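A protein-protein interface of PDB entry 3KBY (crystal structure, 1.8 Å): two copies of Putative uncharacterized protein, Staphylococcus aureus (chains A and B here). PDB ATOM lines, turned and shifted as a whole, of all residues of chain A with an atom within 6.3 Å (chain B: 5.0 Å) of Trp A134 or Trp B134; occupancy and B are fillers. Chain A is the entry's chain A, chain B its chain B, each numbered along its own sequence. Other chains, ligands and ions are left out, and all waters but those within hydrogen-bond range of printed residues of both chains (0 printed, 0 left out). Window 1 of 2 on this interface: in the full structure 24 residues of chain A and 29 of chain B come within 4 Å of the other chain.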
ATOM      1  N   ILE A 127      24.345  20.760   8.574  1.00  0.00           N
ATOM      2  CA  ILE A 127      23.178  20.080   9.165  1.00  0.00           C
ATOM      3  C   ILE A 127      23.011  18.662   8.620  1.00  0.00           C
ATOM      4  O   ILE A 127      22.784  17.719   9.385  1.00  0.00           O
ATOM      5  CB  ILE A 127      21.881  20.912   8.985  1.00  0.00           C
ATOM      6  CG1 ILE A 127      21.956  22.194   9.827  1.00  0.00           C
ATOM      7  CG2 ILE A 127      20.643  20.089   9.381  1.00  0.00           C
ATOM      8  CD1 ILE A 127      20.747  23.141   9.637  1.00  0.00           C
ATOM      9  N   GLN A 129      25.250  16.727   7.405  1.00  0.00           N
ATOM     10  CA  GLN A 129      26.332  15.904   7.950  1.00  0.00           C
ATOM     11  C   GLN A 129      26.077  15.546   9.417  1.00  0.00           C
ATOM     12  O   GLN A 129      26.404  14.445   9.856  1.00  0.00           O
ATOM     13  CB  GLN A 129      27.669  16.615   7.738  1.00  0.00           C
ATOM     14  CG  GLN A 129      28.093  16.592   6.256  1.00  0.00           C
ATOM     15  CD  GLN A 129      28.880  17.816   5.811  1.00  0.00           C
ATOM     16  OE1 GLN A 129      29.344  18.617   6.623  1.00  0.00           O
ATOM     17  NE2 GLN A 129      29.033  17.959   4.500  1.00  0.00           N
ATOM     18  N   MET A 130      25.462  16.458  10.166  1.00  0.00           N
ATOM     19  CA  MET A 130      25.062  16.136  11.541  1.00  0.00           C
ATOM     20  C   MET A 130      24.000  15.042  11.557  1.00  0.00           C
ATOM     21  O   MET A 130      24.045  14.140  12.403  1.00  0.00           O
ATOM     22  CB  MET A 130      24.569  17.375  12.301  1.00  0.00           C
ATOM     23  CG  MET A 130      25.656  18.370  12.628  1.00  0.00           C
ATOM     24  SD  MET A 130      27.209  17.610  13.550  1.00  0.00           S
ATOM     25  CE  MET A 130      26.330  17.083  15.226  1.00  0.00           C
ATOM     26  N   ARG A 131      23.033  15.120  10.637  1.00  0.00           N
ATOM     27  CA  ARG A 131      21.973  14.099  10.571  1.00  0.00           C
ATOM     28  C   ARG A 131      22.570  12.712  10.276  1.00  0.00           C
ATOM     29  O   ARG A 131      22.149  11.700  10.836  1.00  0.00           O
ATOM     30  CB  ARG A 131      20.912  14.459   9.508  1.00  0.00           C
ATOM     31  CG  ARG A 131      20.067  15.724   9.799  1.00  0.00           C
ATOM     32  CD  ARG A 131      19.257  15.627  11.095  1.00  0.00           C
ATOM     33  NE  ARG A 131      18.334  14.489  11.156  1.00  0.00           N
ATOM     34  CZ  ARG A 131      17.037  14.542  10.850  1.00  0.00           C
ATOM     35  NH1 ARG A 131      16.477  15.674  10.422  1.00  0.00           N
ATOM     36  NH2 ARG A 131      16.293  13.450  10.978  1.00  0.00           N
ATOM     37  N   ILE A 132      23.545  12.675   9.374  1.00  0.00           N
ATOM     38  CA  ILE A 132      24.263  11.433   9.075  1.00  0.00           C
ATOM     39  C   ILE A 132      24.989  10.925  10.316  1.00  0.00           C
ATOM     40  O   ILE A 132      24.829   9.769  10.702  1.00  0.00           O
ATOM     41  CB  ILE A 132      25.262  11.613   7.913  1.00  0.00           C
ATOM     42  CG1 ILE A 132      24.515  11.925   6.595  1.00  0.00           C
ATOM     43  CG2 ILE A 132      26.157  10.379   7.757  1.00  0.00           C
ATOM     44  CD1 ILE A 132      25.432  12.539   5.527  1.00  0.00           C
ATOM     45  N   PHE A 133      25.745  11.807  10.967  1.00  0.00           N
ATOM     46  CA  PHE A 133      26.501  11.450  12.178  1.00  0.00           C
ATOM     47  C   PHE A 133      25.572  10.882  13.261  1.00  0.00           C
ATOM     48  O   PHE A 133      25.858   9.824  13.833  1.00  0.00           O
ATOM     49  CB  PHE A 133      27.264  12.684  12.695  1.00  0.00           C
ATOM     50  CG  PHE A 133      28.042  12.437  13.964  1.00  0.00           C
ATOM     51  CD1 PHE A 133      29.134  11.577  13.964  1.00  0.00           C
ATOM     52  CD2 PHE A 133      27.677  13.080  15.149  1.00  0.00           C
ATOM     53  CE1 PHE A 133      29.874  11.344  15.162  1.00  0.00           C
ATOM     54  CE2 PHE A 133      28.395  12.862  16.347  1.00  0.00           C
ATOM     55  CZ  PHE A 133      29.497  11.996  16.348  1.00  0.00           C
ATOM     56  N   TRP A 134      24.454  11.575  13.522  1.00  0.00           N
ATOM     57  CA  TRP A 134      23.520  11.148  14.555  1.00  0.00           C
ATOM     58  C   TRP A 134      22.944   9.779  14.226  1.00  0.00           C
ATOM     59  O   TRP A 134      22.916   8.898  15.073  1.00  0.00           O
ATOM     60  CB  TRP A 134      22.386  12.157  14.757  1.00  0.00           C
ATOM     61  CG  TRP A 134      22.813  13.455  15.375  1.00  0.00           C
ATOM     62  CD1 TRP A 134      23.858  13.666  16.241  1.00  0.00           C
ATOM     63  CD2 TRP A 134      22.189  14.722  15.177  1.00  0.00           C
ATOM     64  NE1 TRP A 134      23.927  15.005  16.583  1.00  0.00           N
ATOM     65  CE2 TRP A 134      22.910  15.674  15.947  1.00  0.00           C
ATOM     66  CE3 TRP A 134      21.088  15.152  14.419  1.00  0.00           C
ATOM     67  CZ2 TRP A 134      22.574  17.031  15.966  1.00  0.00           C
ATOM     68  CZ3 TRP A 134      20.747  16.517  14.445  1.00  0.00           C
ATOM     69  CH2 TRP A 134      21.495  17.433  15.208  1.00  0.00           C
ATOM     70  N   GLN A 135      22.484   9.605  12.998  1.00  0.00           N
ATOM     71  CA  GLN A 135      21.964   8.314  12.582  1.00  0.00           C
ATOM     72  C   GLN A 135      23.014   7.186  12.716  1.00  0.00           C
ATOM     73  O   GLN A 135      22.722   6.108  13.233  1.00  0.00           O
ATOM     74  CB  GLN A 135      21.414   8.388  11.157  1.00  0.00           C
ATOM     75  CG  GLN A 135      20.713   7.101  10.746  1.00  0.00           C
ATOM     76  CD  GLN A 135      19.540   6.771  11.656  1.00  0.00           C
ATOM     77  OE1 GLN A 135      18.482   7.377  11.551  1.00  0.00           O
ATOM     78  NE2 GLN A 135      19.733   5.816  12.564  1.00  0.00           N
ATOM     79  N   TYR A 136      24.236   7.463  12.281  1.00  0.00           N
ATOM     80  CA  TYR A 136      25.350   6.522  12.419  1.00  0.00           C
ATOM     81  C   TYR A 136      25.526   6.120  13.886  1.00  0.00           C
ATOM     82  O   TYR A 136      25.596   4.930  14.204  1.00  0.00           O
ATOM     83  CB  TYR A 136      26.658   7.130  11.875  1.00  0.00           C
ATOM     84  CG  TYR A 136      27.868   6.311  12.254  1.00  0.00           C
ATOM     85  CD1 TYR A 136      28.118   5.078  11.642  1.00  0.00           C
ATOM     86  CD2 TYR A 136      28.723   6.737  13.267  1.00  0.00           C
ATOM     87  CE1 TYR A 136      29.242   4.307  12.008  1.00  0.00           C
ATOM     88  CE2 TYR A 136      29.826   5.990  13.649  1.00  0.00           C
ATOM     89  CZ  TYR A 136      30.073   4.768  13.021  1.00  0.00           C
ATOM     90  OH  TYR A 136      31.151   4.004  13.426  1.00  0.00           O
ATOM     91  N   THR A 137      25.629   7.113  14.773  1.00  0.00           N
ATOM     92  CA  THR A 137      25.845   6.823  16.198  1.00  0.00           C
ATOM     93  C   THR A 137      24.688   6.024  16.829  1.00  0.00           C
ATOM     94  O   THR A 137      24.921   5.205  17.718  1.00  0.00           O
ATOM     95  CB  THR A 137      26.159   8.100  17.050  1.00  0.00           C
ATOM     96  OG1 THR A 137      25.068   9.029  16.974  1.00  0.00           O
ATOM     97  CG2 THR A 137      27.434   8.753  16.581  1.00  0.00           C
ATOM     98  N   ALA A 138      23.458   6.245  16.349  1.00  0.00           N
ATOM     99  CA  ALA A 138      22.292   5.555  16.886  1.00  0.00           C
ATOM    100  C   ALA A 138      22.339   4.087  16.492  1.00  0.00           C
ATOM    101  O   ALA A 138      21.929   3.227  17.271  1.00  0.00           O
ATOM    102  CB  ALA A 138      20.998   6.209  16.402  1.00  0.00           C
ATOM    103  N   ILE A 139      22.886   3.807  15.306  1.00  0.00           N
ATOM    104  CA  ILE A 139      23.095   2.421  14.844  1.00  0.00           C
ATOM    105  C   ILE A 139      24.157   1.719  15.695  1.00  0.00           C
ATOM    106  O   ILE A 139      23.939   0.615  16.209  1.00  0.00           O
ATOM    107  CB  ILE A 139      23.460   2.360  13.351  1.00  0.00           C
ATOM    108  CG1 ILE A 139      22.263   2.789  12.481  1.00  0.00           C
ATOM    109  CG2 ILE A 139      23.929   0.951  12.971  1.00  0.00           C
ATOM    110  CD1 ILE A 139      22.648   3.128  11.039  1.00  0.00           C
ATOM    111  N   ARG A 141      25.094   2.355  18.655  1.00  0.00           N
ATOM    112  CA  ARG A 141      24.643   2.163  20.034  1.00  0.00           C
ATOM    113  C   ARG A 141      23.238   1.560  20.120  1.00  0.00           C
ATOM    114  O   ARG A 141      22.515   1.787  21.096  1.00  0.00           O
ATOM    115  CB  ARG A 141      24.727   3.488  20.804  1.00  0.00           C
ATOM    116  CG  ARG A 141      26.152   3.858  21.219  1.00  0.00           C
ATOM    117  CD  ARG A 141      26.527   3.235  22.563  1.00  0.00           C
ATOM    118  NE  ARG A 141      26.950   1.845  22.417  1.00  0.00           N
ATOM    119  CZ  ARG A 141      26.712   0.890  23.306  1.00  0.00           C
ATOM    120  NH1 ARG A 141      26.028   1.155  24.414  1.00  0.00           N
ATOM    121  NH2 ARG A 141      27.157  -0.340  23.082  1.00  0.00           N
ATOM    122  N   MET B   4      13.685  12.712  17.940  1.00  0.00           N
ATOM    123  CA  MET B   4      14.694  13.554  18.574  1.00  0.00           C
ATOM    124  C   MET B   4      15.589  14.206  17.523  1.00  0.00           C
ATOM    125  O   MET B   4      15.912  15.383  17.633  1.00  0.00           O
ATOM    126  CB  MET B   4      15.542  12.796  19.592  1.00  0.00           C
ATOM    127  CG  MET B   4      16.408  13.774  20.383  1.00  0.00           C
ATOM    128  SD  MET B   4      17.390  12.862  21.739  1.00  0.00           S
ATOM    129  CE  MET B   4      18.425  14.401  22.339  1.00  0.00           C
ATOM    130  N   PHE B   5      15.993  13.454  16.505  1.00  0.00           N
ATOM    131  CA  PHE B   5      16.910  14.029  15.517  1.00  0.00           C
ATOM    132  C   PHE B   5      16.241  15.131  14.702  1.00  0.00           C
ATOM    133  O   PHE B   5      16.903  16.115  14.330  1.00  0.00           O
ATOM    134  CB  PHE B   5      17.542  12.969  14.609  1.00  0.00           C
ATOM    135  CG  PHE B   5      18.406  11.967  15.354  1.00  0.00           C
ATOM    136  CD1 PHE B   5      19.033  12.322  16.545  1.00  0.00           C
ATOM    137  CD2 PHE B   5      18.594  10.694  14.849  1.00  0.00           C
ATOM    138  CE1 PHE B   5      19.833  11.406  17.248  1.00  0.00           C
ATOM    139  CE2 PHE B   5      19.400   9.764  15.551  1.00  0.00           C
ATOM    140  CZ  PHE B   5      20.007  10.132  16.740  1.00  0.00           C
ATOM    141  N   LEU B   8      16.332  18.146  17.113  1.00  0.00           N
ATOM    142  CA  LEU B   8      17.652  18.783  17.101  1.00  0.00           C
ATOM    143  C   LEU B   8      17.951  19.564  15.813  1.00  0.00           C
ATOM    144  O   LEU B   8      18.541  20.644  15.879  1.00  0.00           O
ATOM    145  CB  LEU B   8      18.758  17.749  17.347  1.00  0.00           C
ATOM    146  CG  LEU B   8      18.684  16.919  18.618  1.00  0.00           C
ATOM    147  CD1 LEU B   8      19.928  16.031  18.710  1.00  0.00           C
ATOM    148  CD2 LEU B   8      18.558  17.792  19.872  1.00  0.00           C
ATOM    149  N   GLU B   9      17.569  19.040  14.645  1.00  0.00           N
ATOM    150  CA  GLU B   9      17.749  19.828  13.424  1.00  0.00           C
ATOM    151  C   GLU B   9      16.960  21.153  13.484  1.00  0.00           C
ATOM    152  O   GLU B   9      17.464  22.222  13.091  1.00  0.00           O
ATOM    153  CB  GLU B   9      17.373  19.036  12.169  1.00  0.00           C
ATOM    154  CG  GLU B   9      17.373  19.947  10.938  1.00  0.00           C
ATOM    155  CD  GLU B   9      17.390  19.232   9.604  1.00  0.00           C
ATOM    156  OE1 GLU B   9      17.562  18.001   9.558  1.00  0.00           O
ATOM    157  OE2 GLU B   9      17.232  19.937   8.578  1.00  0.00           O
ATOM    158  N   ILE B  12      18.852  23.725  15.475  1.00  0.00           N
ATOM    159  CA  ILE B  12      19.976  24.329  14.754  1.00  0.00           C
ATOM    160  C   ILE B  12      19.445  25.308  13.710  1.00  0.00           C
ATOM    161  O   ILE B  12      19.916  26.440  13.624  1.00  0.00           O
ATOM    162  CB  ILE B  12      20.880  23.279  14.085  1.00  0.00           C
ATOM    163  CG1 ILE B  12      21.542  22.398  15.162  1.00  0.00           C
ATOM    164  CG2 ILE B  12      21.947  23.970  13.190  1.00  0.00           C
ATOM    165  CD1 ILE B  12      22.359  21.219  14.600  1.00  0.00           C
ATOM    166  N   MET B 130      23.292   8.747  25.613  1.00  0.00           N
ATOM    167  CA  MET B 130      23.288   9.076  24.170  1.00  0.00           C
ATOM    168  C   MET B 130      22.483  10.353  23.903  1.00  0.00           C
ATOM    169  O   MET B 130      22.886  11.210  23.102  1.00  0.00           O
ATOM    170  CB  MET B 130      22.754   7.929  23.302  1.00  0.00           C
ATOM    171  CG  MET B 130      23.651   6.692  23.239  1.00  0.00           C
ATOM    172  SD  MET B 130      25.443   7.158  22.637  1.00  0.00           S
ATOM    173  CE  MET B 130      25.070   7.798  20.847  1.00  0.00           C
ATOM    174  N   ARG B 131      21.343  10.482  24.580  1.00  0.00           N
ATOM    175  CA  ARG B 131      20.495  11.644  24.381  1.00  0.00           C
ATOM    176  C   ARG B 131      21.195  12.911  24.872  1.00  0.00           C
ATOM    177  O   ARG B 131      21.133  13.954  24.222  1.00  0.00           O
ATOM    178  CB  ARG B 131      19.134  11.435  25.055  1.00  0.00           C
ATOM    179  CG  ARG B 131      18.297  10.375  24.355  1.00  0.00           C
ATOM    180  CD  ARG B 131      16.923  10.209  24.998  1.00  0.00           C
ATOM    181  NE  ARG B 131      16.040   9.558  24.048  1.00  0.00           N
ATOM    182  CZ  ARG B 131      14.738   9.378  24.249  1.00  0.00           C
ATOM    183  NH1 ARG B 131      14.177   9.766  25.387  1.00  0.00           N
ATOM    184  NH2 ARG B 131      14.004   8.799  23.311  1.00  0.00           N
ATOM    185  N   ILE B 132      21.893  12.810  26.000  1.00  0.00           N
ATOM    186  CA  ILE B 132      22.694  13.946  26.513  1.00  0.00           C
ATOM    187  C   ILE B 132      23.741  14.309  25.461  1.00  0.00           C
ATOM    188  O   ILE B 132      23.890  15.478  25.105  1.00  0.00           O
ATOM    189  CB  ILE B 132      23.433  13.584  27.838  1.00  0.00           C
ATOM    190  CG1 ILE B 132      22.423  13.315  28.974  1.00  0.00           C
ATOM    191  CG2 ILE B 132      24.437  14.673  28.223  1.00  0.00           C
ATOM    192  CD1 ILE B 132      23.032  12.608  30.175  1.00  0.00           C
ATOM    193  N   PHE B 133      24.456  13.290  24.973  1.00  0.00           N
ATOM    194  CA  PHE B 133      25.476  13.476  23.953  1.00  0.00           C
ATOM    195  C   PHE B 133      24.888  14.169  22.711  1.00  0.00           C
ATOM    196  O   PHE B 133      25.446  15.163  22.227  1.00  0.00           O
ATOM    197  CB  PHE B 133      26.128  12.131  23.587  1.00  0.00           C
ATOM    198  CG  PHE B 133      27.145  12.220  22.463  1.00  0.00           C
ATOM    199  CD1 PHE B 133      28.342  12.906  22.638  1.00  0.00           C
ATOM    200  CD2 PHE B 133      26.900  11.595  21.245  1.00  0.00           C
ATOM    201  CE1 PHE B 133      29.296  12.984  21.605  1.00  0.00           C
ATOM    202  CE2 PHE B 133      27.852  11.675  20.178  1.00  0.00           C
ATOM    203  CZ  PHE B 133      29.043  12.364  20.366  1.00  0.00           C
ATOM    204  N   TRP B 134      23.765  13.663  22.214  1.00  0.00           N
ATOM    205  CA  TRP B 134      23.161  14.230  21.004  1.00  0.00           C
ATOM    206  C   TRP B 134      22.723  15.680  21.209  1.00  0.00           C
ATOM    207  O   TRP B 134      22.997  16.548  20.368  1.00  0.00           O
ATOM    208  CB  TRP B 134      21.993  13.378  20.509  1.00  0.00           C
ATOM    209  CG  TRP B 134      22.417  12.047  19.955  1.00  0.00           C
ATOM    210  CD1 TRP B 134      23.539  11.780  19.192  1.00  0.00           C
ATOM    211  CD2 TRP B 134      21.701  10.816  20.061  1.00  0.00           C
ATOM    212  NE1 TRP B 134      23.558  10.446  18.840  1.00  0.00           N
ATOM    213  CE2 TRP B 134      22.449   9.832  19.366  1.00  0.00           C
ATOM    214  CE3 TRP B 134      20.498  10.442  20.682  1.00  0.00           C
ATOM    215  CZ2 TRP B 134      22.026   8.492  19.269  1.00  0.00           C
ATOM    216  CZ3 TRP B 134      20.082   9.093  20.597  1.00  0.00           C
ATOM    217  CH2 TRP B 134      20.849   8.147  19.892  1.00  0.00           C
ATOM    218  N   GLN B 135      22.050  15.943  22.324  1.00  0.00           N
ATOM    219  CA  GLN B 135      21.628  17.314  22.610  1.00  0.00           C
ATOM    220  C   GLN B 135      22.828  18.265  22.774  1.00  0.00           C
ATOM    221  O   GLN B 135      22.805  19.404  22.264  1.00  0.00           O
ATOM    222  CB  GLN B 135      20.706  17.368  23.822  1.00  0.00           C
ATOM    223  CG  GLN B 135      20.284  18.784  24.196  1.00  0.00           C
ATOM    224  CD  GLN B 135      19.366  19.402  23.155  1.00  0.00           C
ATOM    225  OE1 GLN B 135      18.170  19.118  23.139  1.00  0.00           O
ATOM    226  NE2 GLN B 135      19.923  20.242  22.282  1.00  0.00           N
ATOM    227  N   TYR B 136      23.875  17.785  23.451  1.00  0.00           N
ATOM    228  CA  TYR B 136      25.148  18.514  23.506  1.00  0.00           C
ATOM    229  C   TYR B 136      25.678  18.874  22.106  1.00  0.00           C
ATOM    230  O   TYR B 136      25.983  20.044  21.830  1.00  0.00           O
ATOM    231  CB  TYR B 136      26.216  17.714  24.317  1.00  0.00           C
ATOM    232  CG  TYR B 136      27.622  18.258  24.144  1.00  0.00           C
ATOM    233  CD1 TYR B 136      28.053  19.354  24.881  1.00  0.00           C
ATOM    234  CD2 TYR B 136      28.507  17.697  23.218  1.00  0.00           C
ATOM    235  CE1 TYR B 136      29.354  19.885  24.712  1.00  0.00           C
ATOM    236  CE2 TYR B 136      29.800  18.195  23.041  1.00  0.00           C
ATOM    237  CZ  TYR B 136      30.222  19.291  23.781  1.00  0.00           C
ATOM    238  OH  TYR B 136      31.498  19.809  23.600  1.00  0.00           O
ATOM    239  N   THR B 137      25.751  17.883  21.214  1.00  0.00           N
ATOM    240  CA  THR B 137      26.283  18.118  19.852  1.00  0.00           C
ATOM    241  C   THR B 137      25.481  19.159  19.037  1.00  0.00           C
ATOM    242  O   THR B 137      26.045  19.898  18.235  1.00  0.00           O
ATOM    243  CB  THR B 137      26.496  16.814  19.021  1.00  0.00           C
ATOM    244  OG1 THR B 137      25.236  16.172  18.765  1.00  0.00           O
ATOM    245  CG2 THR B 137      27.465  15.855  19.734  1.00  0.00           C
ATOM    246  N   ALA B 138      24.175  19.237  19.283  1.00  0.00           N
ATOM    247  CA  ALA B 138      23.309  20.163  18.551  1.00  0.00           C
ATOM    248  C   ALA B 138      23.586  21.594  19.000  1.00  0.00           C
ATOM    249  O   ALA B 138      23.570  22.544  18.200  1.00  0.00           O
ATOM    250  CB  ALA B 138      21.826  19.788  18.749  1.00  0.00           C
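The side-chain hydroxyl (OG1) of Thr A137 is in hydrogen-bond range of the indole nitrogen (NE1) of Trp B134.
The side-chain carboxylate (OE1) of Glu B9 is in salt-bridge range of the guanidinium group (NH1) of Arg A131.
OG1 of Thr B137 sits at hydrogen-bond distance from NE1 of Trp A134, 2.8 Å away.
The backbone carbonyl oxygen (O) of Trp A134 is in hydrogen-bond range of the side-chain hydroxyl (OG1) of Thr A137, 2.9 Å away.
The backbone carbonyl oxygen of Phe A133 lies within hydrogen-bond range of the side-chain hydroxyl of Thr A137.
O of Trp B134 sits at hydrogen-bond distance from OG1 of Thr B137 (2.8 Å).
Among the printed residues, merely in contact across the chains: Ile A127 with Glu B9 (3.4 Å), Trp A134 with Leu B8 (3.5 Å), Trp A134 with Trp B134 (3.5 Å), Trp A134 with Phe B5 (3.6 Å), Arg A141 with Met B130 (3.7 Å), Ala A138 with Trp B134 (3.8 Å), Ile A127 with Ile B12 (3.8 Å), Met A130 with Thr B137 (3.8 Å), Arg A131 with Phe B5 (3.8 Å), Trp A134 with Ile B12 (3.9 Å), Thr A137 with Met B130 (3.96 Å), Trp A134 with Ala B138 (3.99 Å) and Ala A138 with Phe B5 (3.99 Å).
Of the printed residues of chain B, Trp A134 touches Phe B5 (3.6 Å), Leu B8 (3.5 Å), Ile B12 (3.9 Å), Trp B134 (3.5 Å), Thr B137 (2.8 Å) and Ala B138 (3.99 Å).
Met B4 touches none of the printed residues of chain A.
Of the printed residues of chain A, Leu B8 touches Trp A134 (3.5 Å).
Of the printed residues of chain A, Met B130 touches Thr A137 and Arg A141.
Tyr B136 touches none of the printed residues of chain A.
The nearest residue of chain A that does not touch Trp B134 is Phe A133 (5.5 Å).
The nearest printed residue of chain A that does not touch Ile B12 is Met A130 (4.8 Å).
Of the 14 printed residues of chain B, 8 touch a printed residue of chain A.
Hydrophobic or aromatic side chains of chain B within 4 Å of the printed part of chain A: Phe B5, Leu B8, Ile B12, Met B130, Trp B134 and Ala B138.
Of the 13 printed residues of chain A, 7 touch a printed residue of chain B.
Along chain A the printed residues that touch a printed residue of chain B span positions 127 to 141.
Among the printed residues, 16 pairs touch across the chains.
Met A130 touches Thr B137, and with the chains exchanged Thr A137 touches Met B130.
Trp A134 touches its own counterpart, Trp B134.
Trp A134 touches Thr B137, and with the chains exchanged Thr A137 touches Trp B134.
Trp A134 touches Ala B138, and with the chains exchanged Ala A138 touches Trp B134.
Positions printed for both chains: 130, 131, 132, 133, 134, 135, 136, 137 and 138.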
